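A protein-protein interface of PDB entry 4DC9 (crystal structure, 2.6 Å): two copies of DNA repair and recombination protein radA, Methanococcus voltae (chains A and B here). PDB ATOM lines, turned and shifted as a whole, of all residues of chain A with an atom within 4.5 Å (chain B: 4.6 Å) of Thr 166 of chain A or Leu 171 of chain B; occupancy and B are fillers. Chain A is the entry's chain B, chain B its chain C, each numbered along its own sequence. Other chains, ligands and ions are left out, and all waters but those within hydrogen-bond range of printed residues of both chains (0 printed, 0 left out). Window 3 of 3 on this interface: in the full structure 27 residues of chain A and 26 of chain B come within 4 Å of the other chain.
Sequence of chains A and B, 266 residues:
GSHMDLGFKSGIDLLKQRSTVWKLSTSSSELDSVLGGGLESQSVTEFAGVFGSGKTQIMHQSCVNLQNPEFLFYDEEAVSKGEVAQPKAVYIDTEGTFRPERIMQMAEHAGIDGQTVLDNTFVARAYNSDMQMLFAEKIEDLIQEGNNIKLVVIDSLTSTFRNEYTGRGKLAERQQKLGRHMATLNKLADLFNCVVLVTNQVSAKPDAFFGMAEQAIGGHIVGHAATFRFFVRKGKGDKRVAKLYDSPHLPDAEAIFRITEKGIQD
The backbone carbonyl oxygen (O) of Asn 163 of chain A lies within hydrogen-bond range of the side-chain amide nitrogen (NE2) of Gln 175 of chain B (3.4 Å).
The side-chain amide oxygen of Gln 175 of chain B lies within hydrogen-bond range of the guanidinium group of Arg 174 of chain B (2.7 Å).
Among the printed residues, merely in contact across the chains: Thr 166 of chain A with Leu 171 of chain B (3.6 Å), Glu 164 of chain A with Gln 175 of chain B (3.8 Å), Glu 164 of chain A with Ala 172 of chain B (3.8 Å) and Tyr 165 of chain A with Ala 172 of chain B (3.9 Å).
Of the printed residues of chain B, Glu 164 of chain A touches Ala 172 and Gln 175.
Of chain B, only Leu 171 (3.6 Å) comes within 4 Å of Thr 166 of chain A.
Arg 168 of chain B touches none of the printed residues of chain A.
Gly 169 of chain B touches none of the printed residues of chain A.
Of chain A, only Thr 166 (3.6 Å) comes within 4 Å of Leu 171 of chain B.
Printed residues of chain A within 4 Å of Gln 175 of chain B: Asn 163 (3.4 Å) and Glu 164 (3.8 Å).
The nearest printed residue of chain B that does not touch Thr 166 of chain A is Gln 175 of chain B (5.4 Å).
The nearest printed residue of chain B that does not touch Asn 163 of chain A is Leu 171 of chain B (6.5 Å).
Printed residues of chain B that touch a printed residue of chain A: Leu 171, Ala 172 and Gln 175.
Hydrophobic or aromatic side chains of chain B within 4 Å of the printed part of chain A: Leu 171 and Ala 172.
Of the 8 printed residues of chain A, 4 touch a printed residue of chain B.
Printed residues of chain A that touch a printed residue of chain B: Asn 163, Glu 164, Tyr 165 and Thr 166.
Hydrophobic or aromatic side chains of chain A within 4 Å of the printed part of chain B: Tyr 165.
Among the printed residues, 5 pairs touch across the chains.
2 positions are printed for both chains.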
ATOM      1  N   ARG A 162     -18.967  -4.053 -24.188  1.00  0.00           N
ATOM      2  CA  ARG A 162     -20.229  -4.596 -24.572  1.00  0.00           C
ATOM      3  C   ARG A 162     -20.361  -6.031 -24.064  1.00  0.00           C
ATOM      4  O   ARG A 162     -21.465  -6.559 -24.002  1.00  0.00           O
ATOM      5  CB  ARG A 162     -20.465  -4.439 -26.090  1.00  0.00           C
ATOM      6  CG  ARG A 162     -19.867  -5.522 -26.975  1.00  0.00           C
ATOM      7  CD  ARG A 162     -20.388  -5.441 -28.411  1.00  0.00           C
ATOM      8  NE  ARG A 162     -21.719  -6.040 -28.526  1.00  0.00           N
ATOM      9  CZ  ARG A 162     -22.245  -6.560 -29.637  1.00  0.00           C
ATOM     10  NH1 ARG A 162     -23.465  -7.082 -29.590  1.00  0.00           N
ATOM     11  NH2 ARG A 162     -21.567  -6.575 -30.786  1.00  0.00           N
ATOM     12  N   ASN A 163     -19.249  -6.659 -23.685  1.00  0.00           N
ATOM     13  CA  ASN A 163     -19.325  -7.953 -23.022  1.00  0.00           C
ATOM     14  C   ASN A 163     -19.642  -7.833 -21.527  1.00  0.00           C
ATOM     15  O   ASN A 163     -20.251  -8.737 -20.935  1.00  0.00           O
ATOM     16  CB  ASN A 163     -18.048  -8.766 -23.236  1.00  0.00           C
ATOM     17  CG  ASN A 163     -18.006  -9.427 -24.589  1.00  0.00           C
ATOM     18  OD1 ASN A 163     -19.025  -9.499 -25.285  1.00  0.00           O
ATOM     19  ND2 ASN A 163     -16.821  -9.899 -24.986  1.00  0.00           N
ATOM     20  N   GLU A 164     -19.207  -6.727 -20.933  1.00  0.00           N
ATOM     21  CA  GLU A 164     -19.495  -6.403 -19.550  1.00  0.00           C
ATOM     22  C   GLU A 164     -20.910  -5.880 -19.392  1.00  0.00           C
ATOM     23  O   GLU A 164     -21.769  -6.574 -18.838  1.00  0.00           O
ATOM     24  CB  GLU A 164     -18.487  -5.391 -19.033  1.00  0.00           C
ATOM     25  CG  GLU A 164     -17.119  -5.986 -18.797  1.00  0.00           C
ATOM     26  CD  GLU A 164     -16.009  -4.965 -18.856  1.00  0.00           C
ATOM     27  OE1 GLU A 164     -14.888  -5.242 -18.380  1.00  0.00           O
ATOM     28  OE2 GLU A 164     -16.243  -3.872 -19.387  1.00  0.00           O
ATOM     29  N   TYR A 165     -21.161  -4.669 -19.888  1.00  0.00           N
ATOM     30  CA  TYR A 165     -22.484  -4.032 -19.763  1.00  0.00           C
ATOM     31  C   TYR A 165     -23.447  -4.583 -20.774  1.00  0.00           C
ATOM     32  O   TYR A 165     -23.281  -4.407 -21.970  1.00  0.00           O
ATOM     33  CB  TYR A 165     -22.386  -2.528 -19.903  1.00  0.00           C
ATOM     34  CG  TYR A 165     -21.391  -1.930 -18.952  1.00  0.00           C
ATOM     35  CD1 TYR A 165     -21.776  -1.476 -17.692  1.00  0.00           C
ATOM     36  CD2 TYR A 165     -20.049  -1.826 -19.301  1.00  0.00           C
ATOM     37  CE1 TYR A 165     -20.845  -0.935 -16.814  1.00  0.00           C
ATOM     38  CE2 TYR A 165     -19.109  -1.273 -18.431  1.00  0.00           C
ATOM     39  CZ  TYR A 165     -19.506  -0.837 -17.190  1.00  0.00           C
ATOM     40  OH  TYR A 165     -18.544  -0.297 -16.338  1.00  0.00           O
ATOM     41  N   THR A 166     -24.446  -5.278 -20.268  1.00  0.00           N
ATOM     42  CA  THR A 166     -25.440  -5.962 -21.081  1.00  0.00           C
ATOM     43  C   THR A 166     -26.794  -5.493 -20.542  1.00  0.00           C
ATOM     44  O   THR A 166     -26.993  -5.419 -19.312  1.00  0.00           O
ATOM     45  CB  THR A 166     -25.318  -7.511 -20.957  1.00  0.00           C
ATOM     46  OG1 THR A 166     -25.482  -7.904 -19.583  1.00  0.00           O
ATOM     47  CG2 THR A 166     -23.963  -8.036 -21.487  1.00  0.00           C
ATOM     48  N   GLY A 167     -27.694  -5.141 -21.460  1.00  0.00           N
ATOM     49  CA  GLY A 167     -29.053  -4.700 -21.114  1.00  0.00           C
ATOM     50  C   GLY A 167     -29.246  -3.196 -20.970  1.00  0.00           C
ATOM     51  O   GLY A 167     -28.589  -2.402 -21.651  1.00  0.00           O
ATOM     52  N   ARG A 168     -30.166  -2.808 -20.091  1.00  0.00           N
ATOM     53  CA  ARG A 168     -30.377  -1.398 -19.771  1.00  0.00           C
ATOM     54  C   ARG A 168     -29.847  -1.060 -18.353  1.00  0.00           C
ATOM     55  O   ARG A 168     -29.909   0.096 -17.919  1.00  0.00           O
ATOM     56  CB  ARG A 168     -31.861  -1.026 -19.977  1.00  0.00           C
ATOM     57  CG  ARG A 168     -32.253   0.415 -19.647  1.00  0.00           C
ATOM     58  CD  ARG A 168     -33.134   1.044 -20.719  1.00  0.00           C
ATOM     59  NE  ARG A 168     -32.334   1.517 -21.855  1.00  0.00           N
ATOM     60  CZ  ARG A 168     -32.643   2.559 -22.628  1.00  0.00           C
ATOM     61  NH1 ARG A 168     -31.840   2.900 -23.629  1.00  0.00           N
ATOM     62  NH2 ARG A 168     -33.742   3.269 -22.403  1.00  0.00           N
ATOM     63  N   GLY A 169     -29.292  -2.068 -17.668  1.00  0.00           N
ATOM     64  CA  GLY A 169     -28.784  -1.949 -16.285  1.00  0.00           C
ATOM     65  C   GLY A 169     -27.826  -0.806 -15.948  1.00  0.00           C
ATOM     66  O   GLY A 169     -28.200   0.142 -15.248  1.00  0.00           O
ATOM     67  N   ARG B 168     -30.309 -10.691 -12.348  1.00  0.00           N
ATOM     68  CA  ARG B 168     -29.467  -9.905 -13.251  1.00  0.00           C
ATOM     69  C   ARG B 168     -29.720  -8.387 -13.199  1.00  0.00           C
ATOM     70  O   ARG B 168     -29.999  -7.753 -14.217  1.00  0.00           O
ATOM     71  CB  ARG B 168     -29.533 -10.465 -14.690  1.00  0.00           C
ATOM     72  CG  ARG B 168     -30.801 -11.252 -15.034  1.00  0.00           C
ATOM     73  CD  ARG B 168     -30.837 -11.697 -16.494  1.00  0.00           C
ATOM     74  NE  ARG B 168     -30.840 -10.542 -17.410  1.00  0.00           N
ATOM     75  CZ  ARG B 168     -31.881 -10.132 -18.148  1.00  0.00           C
ATOM     76  NH1 ARG B 168     -31.742  -9.062 -18.931  1.00  0.00           N
ATOM     77  NH2 ARG B 168     -33.050 -10.781 -18.125  1.00  0.00           N
ATOM     78  N   GLY B 169     -29.626  -7.824 -11.995  1.00  0.00           N
ATOM     79  CA  GLY B 169     -29.465  -6.381 -11.826  1.00  0.00           C
ATOM     80  C   GLY B 169     -27.979  -6.037 -11.754  1.00  0.00           C
ATOM     81  O   GLY B 169     -27.535  -4.999 -12.269  1.00  0.00           O
ATOM     82  N   LYS B 170     -27.205  -6.925 -11.122  1.00  0.00           N
ATOM     83  CA  LYS B 170     -25.791  -6.673 -10.884  1.00  0.00           C
ATOM     84  C   LYS B 170     -24.888  -7.378 -11.915  1.00  0.00           C
ATOM     85  O   LYS B 170     -23.673  -7.456 -11.711  1.00  0.00           O
ATOM     86  CB  LYS B 170     -25.403  -7.038  -9.432  1.00  0.00           C
ATOM     87  CG  LYS B 170     -25.982  -6.159  -8.305  1.00  0.00           C
ATOM     88  CD  LYS B 170     -27.464  -6.473  -7.986  1.00  0.00           C
ATOM     89  CE  LYS B 170     -27.844  -6.419  -6.499  1.00  0.00           C
ATOM     90  NZ  LYS B 170     -27.533  -5.131  -5.820  1.00  0.00           N
ATOM     91  N   LEU B 171     -25.461  -7.849 -13.029  1.00  0.00           N
ATOM     92  CA  LEU B 171     -24.660  -8.550 -14.064  1.00  0.00           C
ATOM     93  C   LEU B 171     -23.325  -7.910 -14.492  1.00  0.00           C
ATOM     94  O   LEU B 171     -22.328  -8.619 -14.680  1.00  0.00           O
ATOM     95  CB  LEU B 171     -25.457  -8.912 -15.316  1.00  0.00           C
ATOM     96  CG  LEU B 171     -25.643 -10.393 -15.734  1.00  0.00           C
ATOM     97  CD1 LEU B 171     -25.246 -10.601 -17.211  1.00  0.00           C
ATOM     98  CD2 LEU B 171     -24.907 -11.413 -14.850  1.00  0.00           C
ATOM     99  N   ALA B 172     -23.288  -6.591 -14.620  1.00  0.00           N
ATOM    100  CA  ALA B 172     -22.070  -5.959 -15.069  1.00  0.00           C
ATOM    101  C   ALA B 172     -20.917  -6.203 -14.109  1.00  0.00           C
ATOM    102  O   ALA B 172     -19.815  -6.502 -14.544  1.00  0.00           O
ATOM    103  CB  ALA B 172     -22.271  -4.471 -15.303  1.00  0.00           C
ATOM    104  N   GLU B 173     -21.138  -6.063 -12.808  1.00  0.00           N
ATOM    105  CA  GLU B 173     -20.028  -6.312 -11.888  1.00  0.00           C
ATOM    106  C   GLU B 173     -19.612  -7.794 -11.983  1.00  0.00           C
ATOM    107  O   GLU B 173     -18.423  -8.114 -11.929  1.00  0.00           O
ATOM    108  CB  GLU B 173     -20.377  -5.918 -10.462  1.00  0.00           C
ATOM    109  CG  GLU B 173     -19.230  -6.064  -9.476  1.00  0.00           C
ATOM    110  CD  GLU B 173     -19.701  -6.564  -8.109  1.00  0.00           C
ATOM    111  OE1 GLU B 173     -18.947  -7.332  -7.453  1.00  0.00           O
ATOM    112  OE2 GLU B 173     -20.834  -6.211  -7.690  1.00  0.00           O
ATOM    113  N   ARG B 174     -20.584  -8.686 -12.171  1.00  0.00           N
ATOM    114  CA  ARG B 174     -20.265 -10.080 -12.374  1.00  0.00           C
ATOM    115  C   ARG B 174     -19.273 -10.191 -13.519  1.00  0.00           C
ATOM    116  O   ARG B 174     -18.114 -10.578 -13.322  1.00  0.00           O
ATOM    117  CB  ARG B 174     -21.524 -10.892 -12.665  1.00  0.00           C
ATOM    118  CG  ARG B 174     -21.323 -12.390 -12.526  1.00  0.00           C
ATOM    119  CD  ARG B 174     -21.348 -13.087 -13.872  1.00  0.00           C
ATOM    120  NE  ARG B 174     -22.504 -13.978 -13.995  1.00  0.00           N
ATOM    121  CZ  ARG B 174     -22.931 -14.522 -15.135  1.00  0.00           C
ATOM    122  NH1 ARG B 174     -22.303 -14.265 -16.289  1.00  0.00           N
ATOM    123  NH2 ARG B 174     -24.001 -15.325 -15.121  1.00  0.00           N
ATOM    124  N   GLN B 175     -19.730  -9.795 -14.701  1.00  0.00           N
ATOM    125  CA  GLN B 175     -18.942  -9.913 -15.920  1.00  0.00           C
ATOM    126  C   GLN B 175     -17.546  -9.325 -15.807  1.00  0.00           C
ATOM    127  O   GLN B 175     -16.583  -9.927 -16.275  1.00  0.00           O
ATOM    128  CB  GLN B 175     -19.703  -9.322 -17.102  1.00  0.00           C
ATOM    129  CG  GLN B 175     -20.952 -10.117 -17.490  1.00  0.00           C
ATOM    130  CD  GLN B 175     -20.645 -11.531 -18.004  1.00  0.00           C
ATOM    131  OE1 GLN B 175     -20.505 -12.498 -17.229  1.00  0.00           O
ATOM    132  NE2 GLN B 175     -20.582 -11.662 -19.325  1.00  0.00           N
